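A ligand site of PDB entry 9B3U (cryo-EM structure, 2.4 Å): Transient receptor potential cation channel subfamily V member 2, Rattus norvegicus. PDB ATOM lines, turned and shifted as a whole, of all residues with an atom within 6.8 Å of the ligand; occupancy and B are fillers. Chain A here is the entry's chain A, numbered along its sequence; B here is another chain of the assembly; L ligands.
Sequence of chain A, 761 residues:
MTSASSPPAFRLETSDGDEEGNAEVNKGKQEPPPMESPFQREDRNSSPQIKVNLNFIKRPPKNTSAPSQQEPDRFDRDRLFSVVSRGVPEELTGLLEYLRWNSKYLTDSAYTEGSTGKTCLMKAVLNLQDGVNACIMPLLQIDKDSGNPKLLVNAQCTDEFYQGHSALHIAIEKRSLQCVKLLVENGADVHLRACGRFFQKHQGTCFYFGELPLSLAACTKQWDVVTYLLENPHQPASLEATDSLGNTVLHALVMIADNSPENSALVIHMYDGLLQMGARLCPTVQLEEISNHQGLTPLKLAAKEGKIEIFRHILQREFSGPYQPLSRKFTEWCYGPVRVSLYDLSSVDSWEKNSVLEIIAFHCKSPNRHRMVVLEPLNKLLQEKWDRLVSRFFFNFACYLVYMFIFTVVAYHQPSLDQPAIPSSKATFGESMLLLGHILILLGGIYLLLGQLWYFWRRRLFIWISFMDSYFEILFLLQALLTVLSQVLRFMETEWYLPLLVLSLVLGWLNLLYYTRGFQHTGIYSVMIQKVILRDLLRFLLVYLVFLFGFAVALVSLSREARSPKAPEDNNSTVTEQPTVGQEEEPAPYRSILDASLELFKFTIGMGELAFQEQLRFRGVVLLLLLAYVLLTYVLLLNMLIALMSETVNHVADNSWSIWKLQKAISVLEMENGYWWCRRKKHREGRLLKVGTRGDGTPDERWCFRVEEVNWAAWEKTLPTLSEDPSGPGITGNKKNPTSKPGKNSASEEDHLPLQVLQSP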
ATOM      1  N   GLU A 113      11.472  15.940 -34.224  1.00  0.00           N
ATOM      2  CA  GLU A 113      10.017  15.865 -34.478  1.00  0.00           C
ATOM      3  C   GLU A 113       9.247  17.178 -34.186  1.00  0.00           C
ATOM      4  O   GLU A 113       8.082  17.308 -34.564  1.00  0.00           O
ATOM      5  CB  GLU A 113       9.373  14.691 -33.708  1.00  0.00           C
ATOM      6  CG  GLU A 113       9.924  13.317 -34.110  1.00  0.00           C
ATOM      7  CD  GLU A 113       8.845  12.231 -34.303  1.00  0.00           C
ATOM      8  OE1 GLU A 113       8.191  11.829 -33.315  1.00  0.00           O
ATOM      9  OE2 GLU A 113       8.681  11.747 -35.442  1.00  0.00           O
ATOM     10  N   THR A 116       7.873  17.839 -29.814  1.00  0.00           N
ATOM     11  CA  THR A 116       8.501  17.383 -28.565  1.00  0.00           C
ATOM     12  C   THR A 116      10.020  17.621 -28.490  1.00  0.00           C
ATOM     13  O   THR A 116      10.596  17.502 -27.421  1.00  0.00           O
ATOM     14  CB  THR A 116       8.236  15.887 -28.350  1.00  0.00           C
ATOM     15  OG1 THR A 116       8.807  15.174 -29.416  1.00  0.00           O
ATOM     16  CG2 THR A 116       6.762  15.516 -28.318  1.00  0.00           C
ATOM     17  N   LYS A 118      12.114  15.639 -30.145  1.00  0.00           N
ATOM     18  CA  LYS A 118      12.586  14.225 -30.165  1.00  0.00           C
ATOM     19  C   LYS A 118      13.518  14.038 -31.360  1.00  0.00           C
ATOM     20  O   LYS A 118      13.182  14.581 -32.416  1.00  0.00           O
ATOM     21  CB  LYS A 118      11.361  13.335 -30.206  1.00  0.00           C
ATOM     22  CG  LYS A 118      11.528  11.866 -30.615  1.00  0.00           C
ATOM     23  CD  LYS A 118      10.212  11.164 -30.862  1.00  0.00           C
ATOM     24  CE  LYS A 118      10.375   9.783 -31.461  1.00  0.00           C
ATOM     25  NZ  LYS A 118       9.072   9.151 -31.756  1.00  0.00           N
ATOM     26  N   MET A 122      16.535   8.902 -30.863  1.00  0.00           N
ATOM     27  CA  MET A 122      15.333   8.384 -30.187  1.00  0.00           C
ATOM     28  C   MET A 122      14.470   7.564 -31.157  1.00  0.00           C
ATOM     29  O   MET A 122      14.025   6.475 -30.819  1.00  0.00           O
ATOM     30  CB  MET A 122      14.507   9.524 -29.599  1.00  0.00           C
ATOM     31  CG  MET A 122      15.265  10.297 -28.529  1.00  0.00           C
ATOM     32  SD  MET A 122      14.294  11.662 -27.870  1.00  0.00           S
ATOM     33  CE  MET A 122      15.612  12.686 -27.216  1.00  0.00           C
ATOM     34  N   LEU A 126      13.555   3.515 -30.857  1.00  0.00           N
ATOM     35  CA  LEU A 126      12.233   2.964 -31.150  1.00  0.00           C
ATOM     36  C   LEU A 126      12.306   1.955 -32.328  1.00  0.00           C
ATOM     37  O   LEU A 126      13.102   2.105 -33.240  1.00  0.00           O
ATOM     38  CB  LEU A 126      11.244   4.105 -31.440  1.00  0.00           C
ATOM     39  CG  LEU A 126      11.006   5.016 -30.214  1.00  0.00           C
ATOM     40  CD1 LEU A 126      10.293   6.296 -30.633  1.00  0.00           C
ATOM     41  CD2 LEU A 126      10.169   4.306 -29.165  1.00  0.00           C
ATOM     42  N   ASN A 127      11.453   0.919 -32.295  1.00  0.00           N
ATOM     43  CA  ASN A 127      11.438  -0.124 -33.364  1.00  0.00           C
ATOM     44  C   ASN A 127      12.826  -0.761 -33.503  1.00  0.00           C
ATOM     45  O   ASN A 127      13.542  -0.437 -34.473  1.00  0.00           O
ATOM     46  CB  ASN A 127      10.833   0.367 -34.687  1.00  0.00           C
ATOM     47  CG  ASN A 127      11.529   1.570 -35.298  1.00  0.00           C
ATOM     48  OD1 ASN A 127      12.459   1.420 -36.091  1.00  0.00           O
ATOM     49  ND2 ASN A 127      11.081   2.767 -34.937  1.00  0.00           N
ATOM     50  N   CYS A 157      13.734  15.337 -24.945  1.00  0.00           N
ATOM     51  CA  CYS A 157      12.482  16.047 -25.252  1.00  0.00           C
ATOM     52  C   CYS A 157      12.316  17.316 -24.400  1.00  0.00           C
ATOM     53  O   CYS A 157      12.864  17.415 -23.292  1.00  0.00           O
ATOM     54  CB  CYS A 157      11.297  15.089 -25.075  1.00  0.00           C
ATOM     55  SG  CYS A 157      11.418  13.685 -26.213  1.00  0.00           S
ATOM     56  N   TYR A 162       6.673  15.742 -21.977  1.00  0.00           N
ATOM     57  CA  TYR A 162       7.780  14.791 -22.066  1.00  0.00           C
ATOM     58  C   TYR A 162       9.157  15.373 -21.726  1.00  0.00           C
ATOM     59  O   TYR A 162      10.165  14.719 -21.969  1.00  0.00           O
ATOM     60  CB  TYR A 162       7.746  14.034 -23.399  1.00  0.00           C
ATOM     61  CG  TYR A 162       6.374  13.460 -23.717  1.00  0.00           C
ATOM     62  CD1 TYR A 162       5.878  12.372 -22.960  1.00  0.00           C
ATOM     63  CD2 TYR A 162       5.557  14.051 -24.686  1.00  0.00           C
ATOM     64  CE1 TYR A 162       4.584  11.899 -23.171  1.00  0.00           C
ATOM     65  CE2 TYR A 162       4.247  13.579 -24.902  1.00  0.00           C
ATOM     66  CZ  TYR A 162       3.763  12.506 -24.144  1.00  0.00           C
ATOM     67  OH  TYR A 162       2.491  12.066 -24.319  1.00  0.00           O
ATOM     68  N   HIS A 165      12.925  13.553 -21.272  1.00  0.00           N
ATOM     69  CA  HIS A 165      12.896  12.160 -21.796  1.00  0.00           C
ATOM     70  C   HIS A 165      14.084  11.996 -22.730  1.00  0.00           C
ATOM     71  O   HIS A 165      14.402  12.956 -23.400  1.00  0.00           O
ATOM     72  CB  HIS A 165      11.562  11.869 -22.466  1.00  0.00           C
ATOM     73  CG  HIS A 165      11.323  10.451 -22.835  1.00  0.00           C
ATOM     74  ND1 HIS A 165      11.721   9.407 -22.036  1.00  0.00           N
ATOM     75  CD2 HIS A 165      10.698   9.906 -23.898  1.00  0.00           C
ATOM     76  CE1 HIS A 165      11.372   8.273 -22.605  1.00  0.00           C
ATOM     77  NE2 HIS A 165      10.739   8.546 -23.735  1.00  0.00           N
ATOM     78  N   SER A 166      14.667  10.805 -22.814  1.00  0.00           N
ATOM     79  CA  SER A 166      15.921  10.604 -23.550  1.00  0.00           C
ATOM     80  C   SER A 166      16.005   9.226 -24.209  1.00  0.00           C
ATOM     81  O   SER A 166      15.270   8.314 -23.854  1.00  0.00           O
ATOM     82  CB  SER A 166      17.113  10.835 -22.616  1.00  0.00           C
ATOM     83  OG  SER A 166      17.343   9.723 -21.768  1.00  0.00           O
ATOM     84  N   ILE A 170      14.166   5.421 -23.320  1.00  0.00           N
ATOM     85  CA  ILE A 170      13.522   4.603 -24.357  1.00  0.00           C
ATOM     86  C   ILE A 170      14.182   3.217 -24.456  1.00  0.00           C
ATOM     87  O   ILE A 170      13.460   2.217 -24.468  1.00  0.00           O
ATOM     88  CB  ILE A 170      13.486   5.311 -25.720  1.00  0.00           C
ATOM     89  CG1 ILE A 170      12.787   6.678 -25.636  1.00  0.00           C
ATOM     90  CG2 ILE A 170      12.750   4.454 -26.760  1.00  0.00           C
ATOM     91  CD1 ILE A 170      12.979   7.556 -26.879  1.00  0.00           C
ATOM     92  N   GLU A 173      13.002   1.190 -21.333  1.00  0.00           N
ATOM     93  CA  GLU A 173      11.591   0.773 -21.462  1.00  0.00           C
ATOM     94  C   GLU A 173      11.366  -0.236 -22.611  1.00  0.00           C
ATOM     95  O   GLU A 173      10.568  -1.164 -22.472  1.00  0.00           O
ATOM     96  CB  GLU A 173      10.714   2.022 -21.576  1.00  0.00           C
ATOM     97  CG  GLU A 173       9.265   1.833 -22.060  1.00  0.00           C
ATOM     98  CD  GLU A 173       8.465   0.666 -21.455  1.00  0.00           C
ATOM     99  OE1 GLU A 173       8.705   0.302 -20.283  1.00  0.00           O
ATOM    100  OE2 GLU A 173       7.561   0.170 -22.158  1.00  0.00           O
ATOM    101  N   LYS A 174      12.103  -0.146 -23.722  1.00  0.00           N
ATOM    102  CA  LYS A 174      12.104  -1.164 -24.799  1.00  0.00           C
ATOM    103  C   LYS A 174      12.839  -2.460 -24.438  1.00  0.00           C
ATOM    104  O   LYS A 174      12.889  -3.372 -25.252  1.00  0.00           O
ATOM    105  CB  LYS A 174      12.603  -0.540 -26.114  1.00  0.00           C
ATOM    106  CG  LYS A 174      11.601   0.455 -26.737  1.00  0.00           C
ATOM    107  CD  LYS A 174      10.360  -0.259 -27.304  1.00  0.00           C
ATOM    108  CE  LYS A 174       9.337   0.725 -27.879  1.00  0.00           C
ATOM    109  NZ  LYS A 174       8.078   0.033 -28.254  1.00  0.00           N
ATOM    110  N   PHE A 198       3.959  14.097 -18.047  1.00  0.00           N
ATOM    111  CA  PHE A 198       3.685  12.662 -18.220  1.00  0.00           C
ATOM    112  C   PHE A 198       4.413  11.777 -17.195  1.00  0.00           C
ATOM    113  O   PHE A 198       3.926  10.709 -16.836  1.00  0.00           O
ATOM    114  CB  PHE A 198       4.088  12.259 -19.634  1.00  0.00           C
ATOM    115  CG  PHE A 198       3.865  10.785 -19.905  1.00  0.00           C
ATOM    116  CD1 PHE A 198       2.565  10.285 -19.979  1.00  0.00           C
ATOM    117  CD2 PHE A 198       4.965   9.917 -19.976  1.00  0.00           C
ATOM    118  CE1 PHE A 198       2.351   8.902 -20.100  1.00  0.00           C
ATOM    119  CE2 PHE A 198       4.752   8.534 -20.120  1.00  0.00           C
ATOM    120  CZ  PHE A 198       3.455   8.032 -20.184  1.00  0.00           C
ATOM    121  N   PHE A 199       5.567  12.214 -16.702  1.00  0.00           N
ATOM    122  CA  PHE A 199       6.404  11.451 -15.775  1.00  0.00           C
ATOM    123  C   PHE A 199       6.158  11.771 -14.300  1.00  0.00           C
ATOM    124  O   PHE A 199       6.728  11.129 -13.427  1.00  0.00           O
ATOM    125  CB  PHE A 199       7.857  11.695 -16.154  1.00  0.00           C
ATOM    126  CG  PHE A 199       8.153  11.331 -17.584  1.00  0.00           C
ATOM    127  CD1 PHE A 199       8.122   9.987 -17.968  1.00  0.00           C
ATOM    128  CD2 PHE A 199       8.467  12.331 -18.517  1.00  0.00           C
ATOM    129  CE1 PHE A 199       8.429   9.623 -19.291  1.00  0.00           C
ATOM    130  CE2 PHE A 199       8.774  11.967 -19.839  1.00  0.00           C
ATOM    131  CZ  PHE A 199       8.759  10.622 -20.219  1.00  0.00           C
ATOM    132  N   PHE A 207       3.018   8.128 -16.122  1.00  0.00           N
ATOM    133  CA  PHE A 207       3.855   7.017 -15.702  1.00  0.00           C
ATOM    134  C   PHE A 207       4.976   7.559 -14.805  1.00  0.00           C
ATOM    135  O   PHE A 207       6.058   7.909 -15.272  1.00  0.00           O
ATOM    136  CB  PHE A 207       4.375   6.289 -16.944  1.00  0.00           C
ATOM    137  CG  PHE A 207       5.353   5.148 -16.740  1.00  0.00           C
ATOM    138  CD1 PHE A 207       5.332   4.326 -15.595  1.00  0.00           C
ATOM    139  CD2 PHE A 207       6.263   4.853 -17.763  1.00  0.00           C
ATOM    140  CE1 PHE A 207       6.213   3.242 -15.482  1.00  0.00           C
ATOM    141  CE2 PHE A 207       7.152   3.778 -17.650  1.00  0.00           C
ATOM    142  CZ  PHE A 207       7.120   2.964 -16.509  1.00  0.00           C
ATOM    143  N   THR B 331      -3.150   0.950 -32.048  1.00  0.00           N
ATOM    144  CA  THR B 331      -2.182   1.472 -31.071  1.00  0.00           C
ATOM    145  C   THR B 331      -1.342   2.580 -31.698  1.00  0.00           C
ATOM    146  O   THR B 331      -0.805   2.446 -32.791  1.00  0.00           O
ATOM    147  CB  THR B 331      -1.322   0.349 -30.462  1.00  0.00           C
ATOM    148  OG1 THR B 331      -0.596   0.888 -29.392  1.00  0.00           O
ATOM    149  CG2 THR B 331      -0.299  -0.277 -31.403  1.00  0.00           C
ATOM    150  N   GLU B 332      -1.249   3.731 -31.033  1.00  0.00           N
ATOM    151  CA  GLU B 332      -0.492   4.876 -31.496  1.00  0.00           C
ATOM    152  C   GLU B 332       0.901   4.911 -30.877  1.00  0.00           C
ATOM    153  O   GLU B 332       1.892   5.073 -31.587  1.00  0.00           O
ATOM    154  CB  GLU B 332      -1.292   6.148 -31.174  1.00  0.00           C
ATOM    155  CG  GLU B 332      -0.669   7.388 -31.836  1.00  0.00           C
ATOM    156  CD  GLU B 332      -1.575   8.599 -31.697  1.00  0.00           C
ATOM    157  OE1 GLU B 332      -2.164   8.804 -30.617  1.00  0.00           O
ATOM    158  OE2 GLU B 332      -1.695   9.402 -32.654  1.00  0.00           O
ATOM    159  N   TRP B 333       0.990   4.696 -29.567  1.00  0.00           N
ATOM    160  CA  TRP B 333       2.222   4.380 -28.842  1.00  0.00           C
ATOM    161  C   TRP B 333       1.930   3.648 -27.537  1.00  0.00           C
ATOM    162  O   TRP B 333       0.832   3.725 -26.987  1.00  0.00           O
ATOM    163  CB  TRP B 333       3.077   5.638 -28.612  1.00  0.00           C
ATOM    164  CG  TRP B 333       2.467   6.774 -27.836  1.00  0.00           C
ATOM    165  CD1 TRP B 333       1.887   7.856 -28.402  1.00  0.00           C
ATOM    166  CD2 TRP B 333       2.412   6.987 -26.398  1.00  0.00           C
ATOM    167  NE1 TRP B 333       1.506   8.738 -27.413  1.00  0.00           N
ATOM    168  CE2 TRP B 333       1.845   8.277 -26.164  1.00  0.00           C
ATOM    169  CE3 TRP B 333       2.808   6.259 -25.258  1.00  0.00           C
ATOM    170  CZ2 TRP B 333       1.707   8.827 -24.883  1.00  0.00           C
ATOM    171  CZ3 TRP B 333       2.621   6.772 -23.962  1.00  0.00           C
ATOM    172  CH2 TRP B 333       2.085   8.063 -23.771  1.00  0.00           C
ATOM    173  N   CYS B 334       2.920   2.929 -27.017  1.00  0.00           N
ATOM    174  CA  CYS B 334       2.859   2.214 -25.755  1.00  0.00           C
ATOM    175  C   CYS B 334       4.166   2.420 -24.993  1.00  0.00           C
ATOM    176  O   CYS B 334       5.242   2.218 -25.555  1.00  0.00           O
ATOM    177  CB  CYS B 334       2.550   0.749 -26.082  1.00  0.00           C
ATOM    178  SG  CYS B 334       2.351  -0.238 -24.595  1.00  0.00           S
ATOM    179  N   TYR B 335       4.100   2.819 -23.722  1.00  0.00           N
ATOM    180  CA  TYR B 335       5.277   3.120 -22.904  1.00  0.00           C
ATOM    181  C   TYR B 335       4.981   2.791 -21.440  1.00  0.00           C
ATOM    182  O   TYR B 335       4.176   3.441 -20.780  1.00  0.00           O
ATOM    183  CB  TYR B 335       5.686   4.586 -23.102  1.00  0.00           C
ATOM    184  CG  TYR B 335       6.973   4.996 -22.409  1.00  0.00           C
ATOM    185  CD1 TYR B 335       6.939   5.470 -21.092  1.00  0.00           C
ATOM    186  CD2 TYR B 335       8.187   4.943 -23.103  1.00  0.00           C
ATOM    187  CE1 TYR B 335       8.135   5.840 -20.446  1.00  0.00           C
ATOM    188  CE2 TYR B 335       9.386   5.297 -22.453  1.00  0.00           C
ATOM    189  CZ  TYR B 335       9.360   5.752 -21.122  1.00  0.00           C
ATOM    190  OH  TYR B 335      10.514   6.106 -20.501  1.00  0.00           O
HETATM  191  C1  LIG L   1       6.856   3.985 -27.627  1.00  0.00           C
HETATM  192  C2  LIG L   1       6.288   5.114 -29.696  1.00  0.00           C
HETATM  193  C3  LIG L   1       5.756   2.640 -29.481  1.00  0.00           C
HETATM  194  C4  LIG L   1       6.820   8.399 -22.703  1.00  0.00           C
HETATM  195  C5  LIG L   1       6.699   9.049 -24.079  1.00  0.00           C
HETATM  196  C6  LIG L   1       6.474   8.040 -25.206  1.00  0.00           C
HETATM  197  C7  LIG L   1       5.777   9.097 -27.363  1.00  0.00           C
HETATM  198  C8  LIG L   1       4.974  10.244 -26.726  1.00  0.00           C
HETATM  199  C9  LIG L   1       4.153  11.024 -27.764  1.00  0.00           C
HETATM  200  C10 LIG L   1       7.380   6.337 -27.903  1.00  0.00           C
HETATM  201  C11 LIG L   1       7.385   5.180 -27.125  1.00  0.00           C
HETATM  202  C12 LIG L   1       6.301   3.938 -28.927  1.00  0.00           C
HETATM  203  C13 LIG L   1       6.818   6.309 -29.193  1.00  0.00           C
HETATM  204  N1  LIG L   1       6.880   8.623 -26.501  1.00  0.00           N
HETATM  205  O1  LIG L   1       9.130   7.523 -26.245  1.00  0.00           O
HETATM  206  O2  LIG L   1       8.510   8.699 -28.413  1.00  0.00           O
HETATM  207  O3  LIG L   1       5.074   2.689 -30.491  1.00  0.00           O
HETATM  208  O4  LIG L   1       6.058   1.596 -28.926  1.00  0.00           O
HETATM  209  S1  LIG L   1       8.147   7.838 -27.282  1.00  0.00           S
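Residues that only touch the ligand: Cys 334 of chain B (3.2 Å), Phe 198 (3.3 Å), Tyr 335 of chain B (3.3 Å), Trp 333 of chain B (3.4 Å), Leu 126 (3.6 Å), Tyr 162 (3.6 Å), Ile 170 (3.8 Å) and Phe 199 (3.9 Å). Hydrophobic or aromatic side chains within 4 Å of the ligand: Leu 126, Tyr 162, His 165, Ile 170, Phe 198, Phe 199, Trp 333 of chain B and Tyr 335 of chain B. Within 4 Å of the ligand: Lys 118, Leu 126, Tyr 162, His 165, Ile 170, Lys 174, Phe 198, Phe 199, Trp 333 of chain B, Cys 334 of chain B and Tyr 335 of chain B.
OE1 of Glu 113 is in salt-bridge range of NZ of Lys 118. N of Phe 207 lies within hydrogen-bond range of O of Phe 198 (2.8 Å). The side-chain hydroxyl (OG1) of Thr 116 sits close to the backbone NH (N) of Lys 118, 3.4 Å away. The backbone NH (N) of Cys 157 sits at hydrogen-bond distance from the backbone carbonyl oxygen (O) of His 165, 2.9 Å away.
An oxygen (O2) of the ligand lies within hydrogen-bond range of the side-chain amino group (NZ) of Lys 118 (3.4 Å). A ring nitrogen (NE2) of His 165 sits at hydrogen-bond distance from an oxygen (O1) of the ligand, at 3.2 Å. The side-chain amino group (NZ) of Lys 174 is in salt-bridge range of an oxygen (O4) of the ligand, at 2.6 Å.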
